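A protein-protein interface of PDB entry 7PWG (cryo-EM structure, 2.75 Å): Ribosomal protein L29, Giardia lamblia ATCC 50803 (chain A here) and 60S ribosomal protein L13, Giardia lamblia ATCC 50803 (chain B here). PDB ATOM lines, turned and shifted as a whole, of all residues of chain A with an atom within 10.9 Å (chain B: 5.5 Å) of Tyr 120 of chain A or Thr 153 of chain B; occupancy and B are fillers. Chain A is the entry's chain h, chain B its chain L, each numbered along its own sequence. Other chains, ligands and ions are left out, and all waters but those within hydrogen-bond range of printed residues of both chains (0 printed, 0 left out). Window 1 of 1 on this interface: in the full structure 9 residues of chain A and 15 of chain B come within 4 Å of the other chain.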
ATOM      1  N   PRO A 116      17.545 -22.844  -7.097  1.00  0.00           N
ATOM      2  CA  PRO A 116      17.394 -23.248  -8.503  1.00  0.00           C
ATOM      3  C   PRO A 116      18.601 -22.934  -9.380  1.00  0.00           C
ATOM      4  O   PRO A 116      19.677 -22.600  -8.884  1.00  0.00           O
ATOM      5  CB  PRO A 116      16.156 -22.463  -8.956  1.00  0.00           C
ATOM      6  CG  PRO A 116      16.078 -21.300  -8.025  1.00  0.00           C
ATOM      7  CD  PRO A 116      16.578 -21.799  -6.716  1.00  0.00           C
ATOM      8  N   LYS A 117      18.432 -23.095 -10.690  1.00  0.00           N
ATOM      9  CA  LYS A 117      19.456 -22.788 -11.683  1.00  0.00           C
ATOM     10  C   LYS A 117      19.313 -21.340 -12.142  1.00  0.00           C
ATOM     11  O   LYS A 117      18.199 -20.880 -12.408  1.00  0.00           O
ATOM     12  CB  LYS A 117      19.322 -23.739 -12.875  1.00  0.00           C
ATOM     13  CG  LYS A 117      20.560 -23.921 -13.715  1.00  0.00           C
ATOM     14  CD  LYS A 117      20.283 -24.842 -14.900  1.00  0.00           C
ATOM     15  CE  LYS A 117      19.480 -24.149 -16.004  1.00  0.00           C
ATOM     16  NZ  LYS A 117      19.223 -25.041 -17.164  1.00  0.00           N
ATOM     17  N   LEU A 118      20.436 -20.626 -12.234  1.00  0.00           N
ATOM     18  CA  LEU A 118      20.442 -19.194 -12.506  1.00  0.00           C
ATOM     19  C   LEU A 118      21.415 -18.847 -13.622  1.00  0.00           C
ATOM     20  O   LEU A 118      22.524 -19.379 -13.679  1.00  0.00           O
ATOM     21  CB  LEU A 118      20.820 -18.398 -11.255  1.00  0.00           C
ATOM     22  CG  LEU A 118      19.822 -18.453 -10.108  1.00  0.00           C
ATOM     23  CD1 LEU A 118      20.281 -17.593  -8.960  1.00  0.00           C
ATOM     24  CD2 LEU A 118      18.471 -18.003 -10.603  1.00  0.00           C
ATOM     25  N   LYS A 119      20.999 -17.933 -14.489  1.00  0.00           N
ATOM     26  CA  LYS A 119      21.868 -17.368 -15.511  1.00  0.00           C
ATOM     27  C   LYS A 119      22.513 -16.096 -14.977  1.00  0.00           C
ATOM     28  O   LYS A 119      21.865 -15.317 -14.280  1.00  0.00           O
ATOM     29  CB  LYS A 119      21.068 -17.074 -16.787  1.00  0.00           C
ATOM     30  CG  LYS A 119      20.037 -18.133 -17.115  1.00  0.00           C
ATOM     31  CD  LYS A 119      19.900 -18.348 -18.624  1.00  0.00           C
ATOM     32  CE  LYS A 119      19.146 -17.211 -19.321  1.00  0.00           C
ATOM     33  NZ  LYS A 119      19.161 -17.372 -20.809  1.00  0.00           N
ATOM     34  N   TYR A 120      23.799 -15.902 -15.281  1.00  0.00           N
ATOM     35  CA  TYR A 120      24.524 -14.722 -14.818  1.00  0.00           C
ATOM     36  C   TYR A 120      25.701 -14.423 -15.742  1.00  0.00           C
ATOM     37  O   TYR A 120      26.134 -15.274 -16.516  1.00  0.00           O
ATOM     38  CB  TYR A 120      25.005 -14.895 -13.372  1.00  0.00           C
ATOM     39  CG  TYR A 120      25.780 -16.162 -13.122  1.00  0.00           C
ATOM     40  CD1 TYR A 120      27.135 -16.232 -13.382  1.00  0.00           C
ATOM     41  CD2 TYR A 120      25.155 -17.292 -12.622  1.00  0.00           C
ATOM     42  CE1 TYR A 120      27.836 -17.387 -13.167  1.00  0.00           C
ATOM     43  CE2 TYR A 120      25.849 -18.452 -12.413  1.00  0.00           C
ATOM     44  CZ  TYR A 120      27.187 -18.494 -12.680  1.00  0.00           C
ATOM     45  OH  TYR A 120      27.881 -19.651 -12.455  1.00  0.00           O
ATOM     46  N   ALA A 121      26.229 -13.203 -15.648  1.00  0.00           N
ATOM     47  CA  ALA A 121      27.394 -12.808 -16.425  1.00  0.00           C
ATOM     48  C   ALA A 121      28.441 -12.173 -15.525  1.00  0.00           C
ATOM     49  O   ALA A 121      28.113 -11.386 -14.637  1.00  0.00           O
ATOM     50  CB  ALA A 121      27.022 -11.837 -17.548  1.00  0.00           C
ATOM     51  N   VAL A 122      29.701 -12.521 -15.757  1.00  0.00           N
ATOM     52  CA  VAL A 122      30.829 -11.932 -15.046  1.00  0.00           C
ATOM     53  C   VAL A 122      31.497 -10.953 -16.001  1.00  0.00           C
ATOM     54  O   VAL A 122      31.317 -11.043 -17.220  1.00  0.00           O
ATOM     55  CB  VAL A 122      31.815 -13.012 -14.537  1.00  0.00           C
ATOM     56  CG1 VAL A 122      32.847 -12.423 -13.603  1.00  0.00           C
ATOM     57  CG2 VAL A 122      31.080 -14.126 -13.818  1.00  0.00           C
ATOM     58  N   LYS A 123      32.222  -9.990 -15.455  1.00  0.00           N
ATOM     59  CA  LYS A 123      32.902  -8.990 -16.266  1.00  0.00           C
ATOM     60  C   LYS A 123      34.408  -9.042 -16.030  1.00  0.00           C
ATOM     61  O   LYS A 123      34.879  -9.476 -14.977  1.00  0.00           O
ATOM     62  CB  LYS A 123      32.362  -7.596 -15.955  1.00  0.00           C
ATOM     63  CG  LYS A 123      30.854  -7.497 -16.091  1.00  0.00           C
ATOM     64  CD  LYS A 123      30.386  -6.057 -16.149  1.00  0.00           C
ATOM     65  CE  LYS A 123      29.088  -5.843 -15.387  1.00  0.00           C
ATOM     66  NZ  LYS A 123      29.312  -5.927 -13.922  1.00  0.00           N
ATOM     67  N   VAL A 124      35.163  -8.610 -17.036  1.00  0.00           N
ATOM     68  CA  VAL A 124      36.623  -8.572 -16.945  1.00  0.00           C
ATOM     69  C   VAL A 124      37.092  -7.588 -15.878  1.00  0.00           C
ATOM     70  O   VAL A 124      36.286  -6.910 -15.239  1.00  0.00           O
ATOM     71  CB  VAL A 124      37.261  -8.226 -18.299  1.00  0.00           C
ATOM     72  CG1 VAL A 124      37.339  -9.453 -19.172  1.00  0.00           C
ATOM     73  CG2 VAL A 124      36.477  -7.109 -18.995  1.00  0.00           C
ATOM     74  N   PRO B  77      24.864 -16.920 -20.597  1.00  0.00           N
ATOM     75  CA  PRO B  77      26.210 -16.353 -20.627  1.00  0.00           C
ATOM     76  C   PRO B  77      27.086 -16.726 -19.435  1.00  0.00           C
ATOM     77  O   PRO B  77      27.982 -15.959 -19.110  1.00  0.00           O
ATOM     78  CB  PRO B  77      25.931 -14.851 -20.628  1.00  0.00           C
ATOM     79  CG  PRO B  77      24.708 -14.725 -19.780  1.00  0.00           C
ATOM     80  CD  PRO B  77      23.955 -16.058 -19.837  1.00  0.00           C
ATOM     81  N   CYS B  78      26.824 -17.854 -18.783  1.00  0.00           N
ATOM     82  CA  CYS B  78      27.690 -18.272 -17.695  1.00  0.00           C
ATOM     83  C   CYS B  78      29.070 -18.617 -18.245  1.00  0.00           C
ATOM     84  O   CYS B  78      29.184 -19.164 -19.344  1.00  0.00           O
ATOM     85  CB  CYS B  78      27.104 -19.473 -16.954  1.00  0.00           C
ATOM     86  SG  CYS B  78      25.414 -19.233 -16.391  1.00  0.00           S
ATOM     87  N   PRO B  79      30.134 -18.300 -17.520  1.00  0.00           N
ATOM     88  CA  PRO B  79      31.470 -18.727 -17.944  1.00  0.00           C
ATOM     89  C   PRO B  79      31.642 -20.227 -17.764  1.00  0.00           C
ATOM     90  O   PRO B  79      30.850 -20.901 -17.109  1.00  0.00           O
ATOM     91  CB  PRO B  79      32.398 -17.932 -17.034  1.00  0.00           C
ATOM     92  CG  PRO B  79      31.564 -17.628 -15.834  1.00  0.00           C
ATOM     93  CD  PRO B  79      30.172 -17.445 -16.325  1.00  0.00           C
ATOM     94  N   LYS B  82      34.273 -21.945 -12.561  1.00  0.00           N
ATOM     95  CA  LYS B  82      33.875 -21.418 -11.267  1.00  0.00           C
ATOM     96  C   LYS B  82      34.950 -20.477 -10.735  1.00  0.00           C
ATOM     97  O   LYS B  82      36.114 -20.547 -11.122  1.00  0.00           O
ATOM     98  CB  LYS B  82      33.643 -22.560 -10.275  1.00  0.00           C
ATOM     99  CG  LYS B  82      32.648 -23.600 -10.740  1.00  0.00           C
ATOM    100  CD  LYS B  82      31.464 -22.930 -11.422  1.00  0.00           C
ATOM    101  CE  LYS B  82      30.353 -23.908 -11.734  1.00  0.00           C
ATOM    102  NZ  LYS B  82      29.052 -23.348 -11.291  1.00  0.00           N
ATOM    103  N   GLN B 121      25.291 -21.308  -6.173  1.00  0.00           N
ATOM    104  CA  GLN B 121      24.312 -20.954  -7.188  1.00  0.00           C
ATOM    105  C   GLN B 121      24.814 -19.882  -8.144  1.00  0.00           C
ATOM    106  O   GLN B 121      24.395 -19.854  -9.304  1.00  0.00           O
ATOM    107  CB  GLN B 121      23.034 -20.493  -6.503  1.00  0.00           C
ATOM    108  CG  GLN B 121      21.865 -20.347  -7.415  1.00  0.00           C
ATOM    109  CD  GLN B 121      20.584 -20.090  -6.670  1.00  0.00           C
ATOM    110  OE1 GLN B 121      20.587 -19.514  -5.587  1.00  0.00           O
ATOM    111  NE2 GLN B 121      19.476 -20.524  -7.244  1.00  0.00           N
ATOM    112  N   ILE B 122      25.694 -18.993  -7.693  1.00  0.00           N
ATOM    113  CA  ILE B 122      26.160 -17.889  -8.522  1.00  0.00           C
ATOM    114  C   ILE B 122      27.614 -18.073  -8.945  1.00  0.00           C
ATOM    115  O   ILE B 122      28.265 -17.111  -9.347  1.00  0.00           O
ATOM    116  CB  ILE B 122      25.958 -16.534  -7.828  1.00  0.00           C
ATOM    117  CG1 ILE B 122      26.682 -16.515  -6.487  1.00  0.00           C
ATOM    118  CG2 ILE B 122      24.482 -16.230  -7.678  1.00  0.00           C
ATOM    119  CD1 ILE B 122      26.392 -15.301  -5.662  1.00  0.00           C
ATOM    120  N   GLY B 123      28.134 -19.290  -8.868  1.00  0.00           N
ATOM    121  CA  GLY B 123      29.339 -19.647  -9.578  1.00  0.00           C
ATOM    122  C   GLY B 123      30.591 -19.788  -8.761  1.00  0.00           C
ATOM    123  O   GLY B 123      31.676 -19.863  -9.339  1.00  0.00           O
ATOM    124  N   TYR B 148      34.509 -10.146  -6.616  1.00  0.00           N
ATOM    125  CA  TYR B 148      33.759 -10.882  -7.627  1.00  0.00           C
ATOM    126  C   TYR B 148      32.270 -10.580  -7.558  1.00  0.00           C
ATOM    127  O   TYR B 148      31.604 -10.482  -8.594  1.00  0.00           O
ATOM    128  CB  TYR B 148      34.021 -12.374  -7.457  1.00  0.00           C
ATOM    129  CG  TYR B 148      33.180 -13.290  -8.296  1.00  0.00           C
ATOM    130  CD1 TYR B 148      33.470 -13.515  -9.633  1.00  0.00           C
ATOM    131  CD2 TYR B 148      32.111 -13.962  -7.742  1.00  0.00           C
ATOM    132  CE1 TYR B 148      32.699 -14.369 -10.386  1.00  0.00           C
ATOM    133  CE2 TYR B 148      31.340 -14.804  -8.488  1.00  0.00           C
ATOM    134  CZ  TYR B 148      31.634 -15.010  -9.799  1.00  0.00           C
ATOM    135  OH  TYR B 148      30.842 -15.870 -10.508  1.00  0.00           O
ATOM    136  N   LYS B 151      31.403  -7.561  -9.782  1.00  0.00           N
ATOM    137  CA  LYS B 151      31.402  -7.715 -11.226  1.00  0.00           C
ATOM    138  C   LYS B 151      30.488  -8.835 -11.710  1.00  0.00           C
ATOM    139  O   LYS B 151      30.706  -9.360 -12.805  1.00  0.00           O
ATOM    140  CB  LYS B 151      32.828  -7.952 -11.715  1.00  0.00           C
ATOM    141  CG  LYS B 151      33.527  -9.049 -10.974  1.00  0.00           C
ATOM    142  CD  LYS B 151      34.834  -9.394 -11.625  1.00  0.00           C
ATOM    143  CE  LYS B 151      35.877  -8.350 -11.343  1.00  0.00           C
ATOM    144  NZ  LYS B 151      37.110  -8.653 -12.105  1.00  0.00           N
ATOM    145  N   VAL B 152      29.463  -9.194 -10.937  1.00  0.00           N
ATOM    146  CA  VAL B 152      28.503 -10.227 -11.303  1.00  0.00           C
ATOM    147  C   VAL B 152      27.128  -9.593 -11.444  1.00  0.00           C
ATOM    148  O   VAL B 152      26.727  -8.780 -10.606  1.00  0.00           O
ATOM    149  CB  VAL B 152      28.455 -11.365 -10.265  1.00  0.00           C
ATOM    150  CG1 VAL B 152      27.206 -12.170 -10.433  1.00  0.00           C
ATOM    151  CG2 VAL B 152      29.646 -12.259 -10.407  1.00  0.00           C
ATOM    152  N   THR B 153      26.416  -9.961 -12.511  1.00  0.00           N
ATOM    153  CA  THR B 153      25.038  -9.554 -12.752  1.00  0.00           C
ATOM    154  C   THR B 153      24.153 -10.790 -12.896  1.00  0.00           C
ATOM    155  O   THR B 153      24.563 -11.790 -13.484  1.00  0.00           O
ATOM    156  CB  THR B 153      24.936  -8.686 -14.013  1.00  0.00           C
ATOM    157  OG1 THR B 153      23.566  -8.564 -14.409  1.00  0.00           O
ATOM    158  CG2 THR B 153      25.697  -9.306 -15.135  1.00  0.00           C
ATOM    159  N   ILE B 154      22.929 -10.714 -12.379  1.00  0.00           N
ATOM    160  CA  ILE B 154      22.027 -11.862 -12.310  1.00  0.00           C
ATOM    161  C   ILE B 154      20.738 -11.552 -13.059  1.00  0.00           C
ATOM    162  O   ILE B 154      20.073 -10.551 -12.775  1.00  0.00           O
ATOM    163  CB  ILE B 154      21.724 -12.249 -10.854  1.00  0.00           C
ATOM    164  CG1 ILE B 154      22.994 -12.714 -10.155  1.00  0.00           C
ATOM    165  CG2 ILE B 154      20.685 -13.338 -10.791  1.00  0.00           C
ATOM    166  CD1 ILE B 154      22.838 -12.842  -8.670  1.00  0.00           C
ATOM    167  N   PHE B 155      20.370 -12.428 -13.987  1.00  0.00           N
ATOM    168  CA  PHE B 155      19.099 -12.297 -14.687  1.00  0.00           C
ATOM    169  C   PHE B 155      18.037 -13.190 -14.071  1.00  0.00           C
ATOM    170  O   PHE B 155      17.174 -12.728 -13.326  1.00  0.00           O
ATOM    171  CB  PHE B 155      19.271 -12.623 -16.170  1.00  0.00           C
ATOM    172  CG  PHE B 155      20.341 -11.831 -16.833  1.00  0.00           C
ATOM    173  CD1 PHE B 155      20.175 -10.482 -17.059  1.00  0.00           C
ATOM    174  CD2 PHE B 155      21.522 -12.426 -17.213  1.00  0.00           C
ATOM    175  CE1 PHE B 155      21.164  -9.749 -17.665  1.00  0.00           C
ATOM    176  CE2 PHE B 155      22.508 -11.700 -17.819  1.00  0.00           C
ATOM    177  CZ  PHE B 155      22.331 -10.357 -18.048  1.00  0.00           C
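Tyr 120 of chain A touches just these residues of chain B: Pro 77, Cys 78, Pro 79, Gln 121, Ile 122, Gly 123 and Thr 153.
Thr 153 of chain B touches two residues of chain A.
Pro 77 of chain B touches just one residue of chain A: Tyr 120.
Of chain A, only Tyr 120 comes within 4 Å of Pro 79 of chain B.
Of chain A, only Tyr 120 comes within 4 Å of Gly 123 of chain B.
Val 152 of chain B touches just one residue of chain A: Ala 121 (3.6 Å).
Printed residues of chain A within 4 Å of Ile 154 of chain B: Lys 119.
Of the printed residues of chain A, Ile 122 of chain B touches Tyr 120 (3.8 Å).
Of the printed residues of chain B, Val 122 of chain A touches Tyr 148 and Lys 151.
Of the printed residues of chain A, Lys 151 of chain B touches Ala 121, Val 122, Lys 123 and Val 124.
Of the printed residues of chain B, Ala 121 of chain A touches Lys 151 (3.8 Å), Val 152 (3.6 Å) and Thr 153 (3.1 Å).
Lys 82 of chain B touches none of the printed residues of chain A.
Lys 117 of chain A touches none of the printed residues of chain B.
The nearest residue of chain B that does not touch Tyr 120 of chain A is Lys 82 of chain B (4.05 Å).
The nearest printed residue of chain A that does not touch Phe 155 of chain B is Tyr 120 of chain A (4.5 Å).
Hydrophobic or aromatic side chains of chain A that line the printed part of chain B: Pro 116, Leu 118, Tyr 120, Ala 121 and Val 122.
Among the printed residues, 19 pairs touch across the chains.
The backbone carbonyl oxygen (O) of Ile 122 of chain B sits at hydrogen-bond distance from the side-chain hydroxyl (OH) of Tyr 148 of chain B (3.1 Å).
Among the printed residues, merely in contact across the chains: Leu 118 of chain A with Cys 78 of chain B, Leu 118 of chain A with Gln 121 of chain B, Lys 119 of chain A with Ile 154 of chain B, Tyr 120 of chain A with Cys 78 of chain B, Tyr 120 of chain A with Pro 79 of chain B, Tyr 120 of chain A with Gln 121 of chain B, Tyr 120 of chain A with Ile 122 of chain B, Tyr 120 of chain A with Gly 123 of chain B, Tyr 120 of chain A with Thr 153 of chain B, Ala 121 of chain A with Lys 151 of chain B, Ala 121 of chain A with Val 152 of chain B, Val 122 of chain A with Tyr 148 of chain B, Val 122 of chain A with Lys 151 of chain B and Val 124 of chain A with Lys 151 of chain B.
NE2 of Gln 121 of chain B sits at hydrogen-bond distance from O of Pro 116 of chain A, at 2.7 Å.
N of Lys 123 of chain A is in hydrogen-bond range of O of Lys 151 of chain B (3.1 Å).
The backbone carbonyl oxygen (O) of Ala 121 of chain A sits at hydrogen-bond distance from the backbone NH (N) of Thr 153 of chain B.
The backbone carbonyl oxygen (O) of Lys 119 of chain A lies within hydrogen-bond range of the backbone NH (N) of Phe 155 of chain B (3.3 Å).
O of Tyr 120 of chain A lies close to O of Pro 77 of chain B (3.3 Å).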
